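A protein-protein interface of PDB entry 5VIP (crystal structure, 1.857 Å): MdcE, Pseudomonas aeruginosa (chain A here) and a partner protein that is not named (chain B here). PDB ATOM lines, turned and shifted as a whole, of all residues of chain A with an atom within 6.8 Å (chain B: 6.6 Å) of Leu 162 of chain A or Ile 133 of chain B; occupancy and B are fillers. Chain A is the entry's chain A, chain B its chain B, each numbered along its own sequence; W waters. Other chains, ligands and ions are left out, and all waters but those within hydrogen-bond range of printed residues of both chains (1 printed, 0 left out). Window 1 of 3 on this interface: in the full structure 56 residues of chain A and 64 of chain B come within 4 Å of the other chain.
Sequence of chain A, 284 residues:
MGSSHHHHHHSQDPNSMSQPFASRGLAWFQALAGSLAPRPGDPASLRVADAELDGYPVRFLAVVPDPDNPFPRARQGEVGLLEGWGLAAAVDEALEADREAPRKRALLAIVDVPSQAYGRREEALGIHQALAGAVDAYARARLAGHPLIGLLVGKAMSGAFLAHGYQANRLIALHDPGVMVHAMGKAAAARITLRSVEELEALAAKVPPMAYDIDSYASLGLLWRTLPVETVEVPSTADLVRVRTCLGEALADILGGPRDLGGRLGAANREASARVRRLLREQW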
ATOM      1  N   VAL A 113       8.629 -17.532  13.467  1.00  0.00           N
ATOM      2  CA  VAL A 113       8.796 -17.056  14.834  1.00  0.00           C
ATOM      3  C   VAL A 113       9.292 -15.618  14.821  1.00  0.00           C
ATOM      4  O   VAL A 113      10.295 -15.298  14.171  1.00  0.00           O
ATOM      5  CB  VAL A 113       9.781 -17.949  15.624  1.00  0.00           C
ATOM      6  CG1 VAL A 113       9.124 -19.271  15.967  1.00  0.00           C
ATOM      7  CG2 VAL A 113      11.052 -18.177  14.809  1.00  0.00           C
ATOM      8  N   LEU A 131      16.680 -21.946  25.437  1.00  0.00           N
ATOM      9  CA  LEU A 131      16.920 -21.958  23.993  1.00  0.00           C
ATOM     10  C   LEU A 131      18.152 -22.809  23.680  1.00  0.00           C
ATOM     11  O   LEU A 131      18.194 -23.479  22.657  1.00  0.00           O
ATOM     12  CB  LEU A 131      17.077 -20.540  23.445  1.00  0.00           C
ATOM     13  CG  LEU A 131      15.749 -19.891  23.010  1.00  0.00           C
ATOM     14  CD1 LEU A 131      14.702 -19.932  24.122  1.00  0.00           C
ATOM     15  CD2 LEU A 131      15.990 -18.460  22.543  1.00  0.00           C
ATOM     16  N   ALA A 134      17.072 -26.343  23.301  1.00  0.00           N
ATOM     17  CA  ALA A 134      16.509 -26.640  21.985  1.00  0.00           C
ATOM     18  C   ALA A 134      17.605 -26.853  20.944  1.00  0.00           C
ATOM     19  O   ALA A 134      17.545 -27.792  20.142  1.00  0.00           O
ATOM     20  CB  ALA A 134      15.560 -25.520  21.538  1.00  0.00           C
ATOM     21  N   VAL A 135      18.596 -25.967  20.951  1.00  0.00           N
ATOM     22  CA  VAL A 135      19.719 -26.054  20.018  1.00  0.00           C
ATOM     23  C   VAL A 135      20.482 -27.365  20.213  1.00  0.00           C
ATOM     24  O   VAL A 135      20.801 -28.072  19.250  1.00  0.00           O
ATOM     25  CB  VAL A 135      20.680 -24.840  20.189  1.00  0.00           C
ATOM     26  CG1 VAL A 135      21.964 -25.035  19.408  1.00  0.00           C
ATOM     27  CG2 VAL A 135      19.994 -23.563  19.714  1.00  0.00           C
ATOM     28  N   TYR A 138      18.386 -30.392  18.836  1.00  0.00           N
ATOM     29  CA  TYR A 138      18.401 -30.392  17.379  1.00  0.00           C
ATOM     30  C   TYR A 138      19.764 -30.804  16.809  1.00  0.00           C
ATOM     31  O   TYR A 138      19.854 -31.653  15.904  1.00  0.00           O
ATOM     32  CB  TYR A 138      18.032 -29.011  16.844  1.00  0.00           C
ATOM     33  CG  TYR A 138      16.558 -28.753  16.611  1.00  0.00           C
ATOM     34  CD1 TYR A 138      15.839 -29.497  15.677  1.00  0.00           C
ATOM     35  CD2 TYR A 138      15.905 -27.708  17.270  1.00  0.00           C
ATOM     36  CE1 TYR A 138      14.494 -29.217  15.414  1.00  0.00           C
ATOM     37  CE2 TYR A 138      14.558 -27.418  17.015  1.00  0.00           C
ATOM     38  CZ  TYR A 138      13.862 -28.181  16.081  1.00  0.00           C
ATOM     39  OH  TYR A 138      12.523 -27.914  15.801  1.00  0.00           O
ATOM     40  N   ALA A 156      11.859 -15.528  10.656  1.00  0.00           N
ATOM     41  CA  ALA A 156      12.861 -16.408  11.243  1.00  0.00           C
ATOM     42  C   ALA A 156      13.870 -15.521  11.942  1.00  0.00           C
ATOM     43  O   ALA A 156      14.915 -15.194  11.373  1.00  0.00           O
ATOM     44  CB  ALA A 156      13.523 -17.277  10.176  1.00  0.00           C
ATOM     45  N   MET A 157      13.554 -15.130  13.176  1.00  0.00           N
ATOM     46  CA  MET A 157      14.263 -14.031  13.814  1.00  0.00           C
ATOM     47  C   MET A 157      15.146 -14.427  14.995  1.00  0.00           C
ATOM     48  O   MET A 157      14.701 -15.130  15.895  1.00  0.00           O
ATOM     49  CB  MET A 157      13.249 -12.992  14.300  1.00  0.00           C
ATOM     50  CG  MET A 157      12.376 -12.446  13.194  1.00  0.00           C
ATOM     51  SD  MET A 157      13.449 -11.366  11.958  1.00  0.00           S
ATOM     52  CE  MET A 157      13.711  -9.842  13.116  1.00  0.00           C
ATOM     53  N   SER A 158      16.383 -13.937  14.990  1.00  0.00           N
ATOM     54  CA  SER A 158      17.200 -13.867  16.204  1.00  0.00           C
ATOM     55  C   SER A 158      17.336 -15.208  16.939  1.00  0.00           C
ATOM     56  O   SER A 158      17.553 -16.247  16.314  1.00  0.00           O
ATOM     57  CB  SER A 158      16.596 -12.810  17.140  1.00  0.00           C
ATOM     58  OG  SER A 158      17.492 -12.461  18.186  1.00  0.00           O
ATOM     59  N   GLY A 159      17.186 -15.179  18.264  1.00  0.00           N
ATOM     60  CA  GLY A 159      17.351 -16.376  19.076  1.00  0.00           C
ATOM     61  C   GLY A 159      16.275 -17.424  18.856  1.00  0.00           C
ATOM     62  O   GLY A 159      16.494 -18.620  19.075  1.00  0.00           O
ATOM     63  N   ALA A 160      15.095 -16.979  18.436  1.00  0.00           N
ATOM     64  CA  ALA A 160      14.021 -17.910  18.119  1.00  0.00           C
ATOM     65  C   ALA A 160      14.420 -18.799  16.953  1.00  0.00           C
ATOM     66  O   ALA A 160      14.193 -20.016  16.991  1.00  0.00           O
ATOM     67  CB  ALA A 160      12.711 -17.150  17.808  1.00  0.00           C
ATOM     68  N   PHE A 161      15.017 -18.209  15.916  1.00  0.00           N
ATOM     69  CA  PHE A 161      15.484 -18.986  14.760  1.00  0.00           C
ATOM     70  C   PHE A 161      16.685 -19.878  15.122  1.00  0.00           C
ATOM     71  O   PHE A 161      16.793 -21.010  14.643  1.00  0.00           O
ATOM     72  CB  PHE A 161      15.845 -18.049  13.588  1.00  0.00           C
ATOM     73  CG  PHE A 161      16.190 -18.766  12.295  1.00  0.00           C
ATOM     74  CD1 PHE A 161      15.691 -20.035  12.016  1.00  0.00           C
ATOM     75  CD2 PHE A 161      17.020 -18.161  11.362  1.00  0.00           C
ATOM     76  CE1 PHE A 161      16.014 -20.688  10.833  1.00  0.00           C
ATOM     77  CE2 PHE A 161      17.341 -18.803  10.167  1.00  0.00           C
ATOM     78  CZ  PHE A 161      16.842 -20.073   9.908  1.00  0.00           C
ATOM     79  N   LEU A 162      17.592 -19.380  15.960  1.00  0.00           N
ATOM     80  CA  LEU A 162      18.716 -20.222  16.402  1.00  0.00           C
ATOM     81  C   LEU A 162      18.188 -21.496  17.075  1.00  0.00           C
ATOM     82  O   LEU A 162      18.700 -22.601  16.847  1.00  0.00           O
ATOM     83  CB  LEU A 162      19.636 -19.453  17.360  1.00  0.00           C
ATOM     84  CG  LEU A 162      20.483 -18.352  16.716  1.00  0.00           C
ATOM     85  CD1 LEU A 162      21.231 -17.527  17.756  1.00  0.00           C
ATOM     86  CD2 LEU A 162      21.463 -18.955  15.714  1.00  0.00           C
ATOM     87  N   ALA A 163      17.132 -21.338  17.872  1.00  0.00           N
ATOM     88  CA  ALA A 163      16.564 -22.448  18.638  1.00  0.00           C
ATOM     89  C   ALA A 163      15.695 -23.359  17.779  1.00  0.00           C
ATOM     90  O   ALA A 163      15.596 -24.554  18.035  1.00  0.00           O
ATOM     91  CB  ALA A 163      15.744 -21.918  19.814  1.00  0.00           C
ATOM     92  N   HIS A 164      15.055 -22.779  16.770  1.00  0.00           N
ATOM     93  CA  HIS A 164      14.075 -23.512  15.980  1.00  0.00           C
ATOM     94  C   HIS A 164      14.317 -23.284  14.498  1.00  0.00           C
ATOM     95  O   HIS A 164      13.781 -22.344  13.909  1.00  0.00           O
ATOM     96  CB  HIS A 164      12.662 -23.079  16.368  1.00  0.00           C
ATOM     97  CG  HIS A 164      11.585 -23.782  15.606  1.00  0.00           C
ATOM     98  ND1 HIS A 164      11.441 -25.154  15.613  1.00  0.00           N
ATOM     99  CD2 HIS A 164      10.585 -23.300  14.828  1.00  0.00           C
ATOM    100  CE1 HIS A 164      10.406 -25.489  14.861  1.00  0.00           C
ATOM    101  NE2 HIS A 164       9.864 -24.384  14.378  1.00  0.00           N
ATOM    102  N   GLY A 165      15.171 -24.117  13.920  1.00  0.00           N
ATOM    103  CA  GLY A 165      15.441 -24.060  12.507  1.00  0.00           C
ATOM    104  C   GLY A 165      16.900 -23.980  12.111  1.00  0.00           C
ATOM    105  O   GLY A 165      17.283 -24.597  11.135  1.00  0.00           O
ATOM    106  N   TYR A 166      17.728 -23.231  12.838  1.00  0.00           N
ATOM    107  CA  TYR A 166      19.027 -22.893  12.267  1.00  0.00           C
ATOM    108  C   TYR A 166      20.050 -24.039  12.399  1.00  0.00           C
ATOM    109  O   TYR A 166      21.154 -23.945  11.864  1.00  0.00           O
ATOM    110  CB  TYR A 166      19.629 -21.646  12.913  1.00  0.00           C
ATOM    111  CG  TYR A 166      20.152 -20.632  11.910  1.00  0.00           C
ATOM    112  CD1 TYR A 166      20.111 -19.270  12.188  1.00  0.00           C
ATOM    113  CD2 TYR A 166      20.575 -21.029  10.639  1.00  0.00           C
ATOM    114  CE1 TYR A 166      20.573 -18.337  11.262  1.00  0.00           C
ATOM    115  CE2 TYR A 166      21.015 -20.097   9.708  1.00  0.00           C
ATOM    116  CZ  TYR A 166      21.020 -18.759  10.032  1.00  0.00           C
ATOM    117  OH  TYR A 166      21.449 -17.820   9.104  1.00  0.00           O
ATOM    118  N   GLN A 167      19.706 -25.125  13.083  1.00  0.00           N
ATOM    119  CA  GLN A 167      20.598 -26.282  13.108  1.00  0.00           C
ATOM    120  C   GLN A 167      20.345 -27.262  11.955  1.00  0.00           C
ATOM    121  O   GLN A 167      20.918 -28.344  11.928  1.00  0.00           O
ATOM    122  CB  GLN A 167      20.475 -27.023  14.442  1.00  0.00           C
ATOM    123  CG  GLN A 167      21.177 -26.327  15.596  1.00  0.00           C
ATOM    124  CD  GLN A 167      22.666 -26.102  15.321  1.00  0.00           C
ATOM    125  OE1 GLN A 167      23.394 -27.036  15.003  1.00  0.00           O
ATOM    126  NE2 GLN A 167      23.114 -24.854  15.440  1.00  0.00           N
ATOM    127  N   LEU B  85      29.708  -9.598  16.959  1.00  0.00           N
ATOM    128  CA  LEU B  85      30.309 -10.544  16.027  1.00  0.00           C
ATOM    129  C   LEU B  85      29.903 -10.273  14.579  1.00  0.00           C
ATOM    130  O   LEU B  85      28.754  -9.937  14.296  1.00  0.00           O
ATOM    131  CB  LEU B  85      29.937 -11.980  16.406  1.00  0.00           C
ATOM    132  CG  LEU B  85      30.605 -12.525  17.678  1.00  0.00           C
ATOM    133  CD1 LEU B  85      30.185 -13.957  17.911  1.00  0.00           C
ATOM    134  CD2 LEU B  85      32.121 -12.432  17.582  1.00  0.00           C
ATOM    135  N   GLY B  90      33.147 -14.195  13.674  1.00  0.00           N
ATOM    136  CA  GLY B  90      32.306 -15.364  13.873  1.00  0.00           C
ATOM    137  C   GLY B  90      32.934 -16.642  13.338  1.00  0.00           C
ATOM    138  O   GLY B  90      32.871 -17.686  13.989  1.00  0.00           O
ATOM    139  N   ALA B  94      34.019 -20.229  15.248  1.00  0.00           N
ATOM    140  CA  ALA B  94      33.456 -21.479  14.735  1.00  0.00           C
ATOM    141  C   ALA B  94      34.551 -22.398  14.216  1.00  0.00           C
ATOM    142  O   ALA B  94      34.561 -23.593  14.515  1.00  0.00           O
ATOM    143  CB  ALA B  94      32.420 -21.190  13.624  1.00  0.00           C
ATOM    144  N   GLY B 120      26.139  -9.098  20.973  1.00  0.00           N
ATOM    145  CA  GLY B 120      25.302  -9.509  19.861  1.00  0.00           C
ATOM    146  C   GLY B 120      26.033  -9.506  18.534  1.00  0.00           C
ATOM    147  O   GLY B 120      27.221  -9.787  18.481  1.00  0.00           O
ATOM    148  N   VAL B 121      25.329  -9.207  17.450  1.00  0.00           N
ATOM    149  CA  VAL B 121      25.983  -9.156  16.148  1.00  0.00           C
ATOM    150  C   VAL B 121      26.088  -7.724  15.629  1.00  0.00           C
ATOM    151  O   VAL B 121      25.383  -6.826  16.088  1.00  0.00           O
ATOM    152  CB  VAL B 121      25.241 -10.026  15.110  1.00  0.00           C
ATOM    153  CG1 VAL B 121      25.100 -11.442  15.631  1.00  0.00           C
ATOM    154  CG2 VAL B 121      23.888  -9.450  14.846  1.00  0.00           C
ATOM    155  N   LEU B 128      25.195 -12.590   8.545  1.00  0.00           N
ATOM    156  CA  LEU B 128      26.434 -13.356   8.556  1.00  0.00           C
ATOM    157  C   LEU B 128      26.862 -13.645   9.986  1.00  0.00           C
ATOM    158  O   LEU B 128      27.322 -14.749  10.286  1.00  0.00           O
ATOM    159  CB  LEU B 128      27.533 -12.610   7.806  1.00  0.00           C
ATOM    160  CG  LEU B 128      27.267 -12.541   6.299  1.00  0.00           C
ATOM    161  CD1 LEU B 128      28.259 -11.608   5.616  1.00  0.00           C
ATOM    162  CD2 LEU B 128      27.336 -13.937   5.701  1.00  0.00           C
ATOM    163  N   GLY B 129      26.708 -12.651  10.862  1.00  0.00           N
ATOM    164  CA  GLY B 129      26.985 -12.838  12.275  1.00  0.00           C
ATOM    165  C   GLY B 129      26.075 -13.897  12.884  1.00  0.00           C
ATOM    166  O   GLY B 129      26.519 -14.731  13.669  1.00  0.00           O
ATOM    167  N   LEU B 130      24.799 -13.870  12.516  1.00  0.00           N
ATOM    168  CA  LEU B 130      23.822 -14.808  13.083  1.00  0.00           C
ATOM    169  C   LEU B 130      24.106 -16.222  12.588  1.00  0.00           C
ATOM    170  O   LEU B 130      24.043 -17.186  13.357  1.00  0.00           O
ATOM    171  CB  LEU B 130      22.383 -14.391  12.726  1.00  0.00           C
ATOM    172  CG  LEU B 130      21.261 -15.157  13.442  1.00  0.00           C
ATOM    173  CD1 LEU B 130      21.347 -14.991  14.976  1.00  0.00           C
ATOM    174  CD2 LEU B 130      19.873 -14.744  12.939  1.00  0.00           C
ATOM    175  N   ALA B 131      24.410 -16.345  11.300  1.00  0.00           N
ATOM    176  CA  ALA B 131      24.756 -17.642  10.726  1.00  0.00           C
ATOM    177  C   ALA B 131      26.001 -18.209  11.410  1.00  0.00           C
ATOM    178  O   ALA B 131      26.071 -19.414  11.690  1.00  0.00           O
ATOM    179  CB  ALA B 131      24.975 -17.519   9.221  1.00  0.00           C
ATOM    180  N   ALA B 132      26.970 -17.343  11.702  1.00  0.00           N
ATOM    181  CA  ALA B 132      28.196 -17.774  12.377  1.00  0.00           C
ATOM    182  C   ALA B 132      27.911 -18.271  13.790  1.00  0.00           C
ATOM    183  O   ALA B 132      28.547 -19.204  14.265  1.00  0.00           O
ATOM    184  CB  ALA B 132      29.204 -16.642  12.414  1.00  0.00           C
ATOM    185  N   ILE B 133      26.969 -17.627  14.466  1.00  0.00           N
ATOM    186  CA  ILE B 133      26.575 -18.074  15.793  1.00  0.00           C
ATOM    187  C   ILE B 133      25.965 -19.477  15.706  1.00  0.00           C
ATOM    188  O   ILE B 133      26.218 -20.316  16.564  1.00  0.00           O
ATOM    189  CB  ILE B 133      25.603 -17.075  16.456  1.00  0.00           C
ATOM    190  CG1 ILE B 133      26.369 -15.797  16.844  1.00  0.00           C
ATOM    191  CG2 ILE B 133      24.940 -17.681  17.691  1.00  0.00           C
ATOM    192  CD1 ILE B 133      25.507 -14.702  17.466  1.00  0.00           C
ATOM    193  N   ALA B 134      25.173 -19.737  14.670  1.00  0.00           N
ATOM    194  CA  ALA B 134      24.614 -21.077  14.511  1.00  0.00           C
ATOM    195  C   ALA B 134      25.733 -22.098  14.280  1.00  0.00           C
ATOM    196  O   ALA B 134      25.657 -23.234  14.759  1.00  0.00           O
ATOM    197  CB  ALA B 134      23.606 -21.113  13.368  1.00  0.00           C
ATOM    198  N   GLU B 135      26.782 -21.687  13.578  1.00  0.00           N
ATOM    199  CA  GLU B 135      27.927 -22.567  13.337  1.00  0.00           C
ATOM    200  C   GLU B 135      28.768 -22.773  14.585  1.00  0.00           C
ATOM    201  O   GLU B 135      29.301 -23.863  14.800  1.00  0.00           O
ATOM    202  CB  GLU B 135      28.816 -22.018  12.205  1.00  0.00           C
ATOM    203  CG  GLU B 135      28.206 -22.220  10.826  1.00  0.00           C
ATOM    204  CD  GLU B 135      28.843 -21.369   9.745  1.00  0.00           C
ATOM    205  OE1 GLU B 135      29.900 -20.740  10.001  1.00  0.00           O
ATOM    206  OE2 GLU B 135      28.273 -21.328   8.629  1.00  0.00           O
ATOM    207  N   ILE B 136      28.917 -21.719  15.385  1.00  0.00           N
ATOM    208  CA  ILE B 136      29.578 -21.836  16.680  1.00  0.00           C
ATOM    209  C   ILE B 136      28.825 -22.801  17.585  1.00  0.00           C
ATOM    210  O   ILE B 136      29.422 -23.659  18.246  1.00  0.00           O
ATOM    211  CB  ILE B 136      29.693 -20.456  17.358  1.00  0.00           C
ATOM    212  CG1 ILE B 136      30.659 -19.592  16.544  1.00  0.00           C
ATOM    213  CG2 ILE B 136      30.121 -20.608  18.816  1.00  0.00           C
ATOM    214  CD1 ILE B 136      30.522 -18.099  16.761  1.00  0.00           C
ATOM    215  N   GLN B 137      27.504 -22.667  17.612  1.00  0.00           N
ATOM    216  CA  GLN B 137      26.681 -23.533  18.454  1.00  0.00           C
ATOM    217  C   GLN B 137      26.799 -24.993  18.015  1.00  0.00           C
ATOM    218  O   GLN B 137      27.013 -25.882  18.847  1.00  0.00           O
ATOM    219  CB  GLN B 137      25.225 -23.061  18.445  1.00  0.00           C
ATOM    220  CG  GLN B 137      25.064 -21.770  19.235  1.00  0.00           C
ATOM    221  CD  GLN B 137      23.717 -21.119  19.036  1.00  0.00           C
ATOM    222  OE1 GLN B 137      22.908 -21.578  18.237  1.00  0.00           O
ATOM    223  NE2 GLN B 137      23.471 -20.043  19.762  1.00  0.00           N
ATOM    224  N   ALA B 138      26.728 -25.229  16.709  1.00  0.00           N
ATOM    225  CA  ALA B 138      26.923 -26.570  16.156  1.00  0.00           C
ATOM    226  C   ALA B 138      28.270 -27.169  16.534  1.00  0.00           C
ATOM    227  O   ALA B 138      28.358 -28.354  16.860  1.00  0.00           O
ATOM    228  CB  ALA B 138      26.790 -26.547  14.620  1.00  0.00           C
ATOM    229  N   GLY B 161      22.836 -11.936  23.909  1.00  0.00           N
ATOM    230  CA  GLY B 161      22.495 -12.228  22.530  1.00  0.00           C
ATOM    231  C   GLY B 161      22.650 -13.702  22.212  1.00  0.00           C
ATOM    232  O   GLY B 161      22.610 -14.558  23.113  1.00  0.00           O
ATOM    233  N   GLY B 162      22.827 -13.994  20.928  1.00  0.00           N
ATOM    234  CA  GLY B 162      22.966 -15.358  20.457  1.00  0.00           C
ATOM    235  C   GLY B 162      24.110 -16.101  21.120  1.00  0.00           C
ATOM    236  O   GLY B 162      24.072 -17.323  21.261  1.00  0.00           O
ATOM    237  N   MET B 163      25.139 -15.377  21.530  1.00  0.00           N
ATOM    238  CA  MET B 163      26.267 -16.050  22.184  1.00  0.00           C
ATOM    239  C   MET B 163      25.941 -16.482  23.619  1.00  0.00           C
ATOM    240  O   MET B 163      26.660 -17.294  24.197  1.00  0.00           O
ATOM    241  CB  MET B 163      27.503 -15.151  22.153  1.00  0.00           C
ATOM    242  CG  MET B 163      28.185 -15.101  20.769  1.00  0.00           C
ATOM    243  SD  MET B 163      28.740 -16.888  20.115  1.00  0.00           S
ATOM    244  CE  MET B 163      30.114 -17.270  21.396  1.00  0.00           C
ATOM    245  N   ILE B 165      23.231 -18.112  24.235  1.00  0.00           N
ATOM    246  CA  ILE B 165      22.704 -19.438  23.954  1.00  0.00           C
ATOM    247  C   ILE B 165      23.888 -20.399  23.788  1.00  0.00           C
ATOM    248  O   ILE B 165      23.842 -21.542  24.249  1.00  0.00           O
ATOM    249  CB  ILE B 165      21.806 -19.426  22.694  1.00  0.00           C
ATOM    250  CG1 ILE B 165      20.596 -18.509  22.926  1.00  0.00           C
ATOM    251  CG2 ILE B 165      21.374 -20.845  22.317  1.00  0.00           C
ATOM    252  CD1 ILE B 165      19.670 -18.345  21.687  1.00  0.00           C
ATOM    253  N   ALA B 166      24.953 -19.922  23.144  1.00  0.00           N
ATOM    254  CA  ALA B 166      26.193 -20.706  23.038  1.00  0.00           C
ATOM    255  C   ALA B 166      26.746 -21.010  24.430  1.00  0.00           C
ATOM    256  O   ALA B 166      27.168 -22.124  24.705  1.00  0.00           O
ATOM    257  CB  ALA B 166      27.238 -19.970  22.198  1.00  0.00           C
HETATM  258  O   HOH W   1      21.353 -22.579  16.128  1.00  0.00           O
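Leu 162 of chain A touches just these residues of chain B: Leu 130, Ile 133, Ala 134, Gln 137 and Gly 162. Of chain A, only Leu 162 (3.7 Å) comes within 4 Å of Ile 133 of chain B. Of the printed residues of chain A, Ala 131 of chain B touches Tyr 166 (3.5 Å). Of the printed residues of chain A, Leu 130 of chain B touches Leu 162 (3.8 Å) and Tyr 166 (3.9 Å). Of the printed residues of chain B, Gln 167 of chain A touches Ala 134 (3.1 Å) and Ala 138 (3.5 Å). Printed residues of chain A within 4 Å of Ile 165 of chain B: Leu 131 (3.8 Å). Gly 90 of chain B touches none of the printed residues of chain A. The nearest residue of chain B that does not touch Leu 162 of chain A is Ile 165 of chain B (4.3 Å).
Water W1 lies within hydrogen-bond range of the backbone carbonyl oxygen (O) of Leu 162 of chain A, the side-chain amide oxygen (OE1) of Gln 137 of chain B and the side-chain amide nitrogen (NE2) of Gln 167 of chain A.
The side-chain amide nitrogen (NE2) of Gln 137 of chain B sits at hydrogen-bond distance from the backbone carbonyl oxygen (O) of Gly 162 of chain B, at 3.2 Å. O of Phe 161 of chain A is in hydrogen-bond range of N of Tyr 166 of chain A (3.0 Å).
The side-chain amide nitrogen (NE2) of Gln 167 of chain A lies within hydrogen-bond range of the backbone carbonyl oxygen (O) of Ala 134 of chain B, 3.1 Å away.
Hydrophobic or aromatic side chains of chain A that line the printed part of chain B: Leu 131, Val 135, Leu 162 and Tyr 166. Along chain B the printed residues that touch a printed residue of chain A span positions 130 to 165.
Among the printed residues, merely in contact across the chains: Leu 131 of chain A with Ile 165 of chain B, Val 135 of chain A with Gln 137 of chain B, Leu 162 of chain A with Leu 130 of chain B, Leu 162 of chain A with Ile 133 of chain B, Leu 162 of chain A with Ala 134 of chain B, Leu 162 of chain A with Gln 137 of chain B, Leu 162 of chain A with Gly 162 of chain B, Tyr 166 of chain A with Leu 130 of chain B, Tyr 166 of chain A with Ala 131 of chain B, Tyr 166 of chain A with Ala 134 of chain B and Gln 167 of chain A with Ala 138 of chain B.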
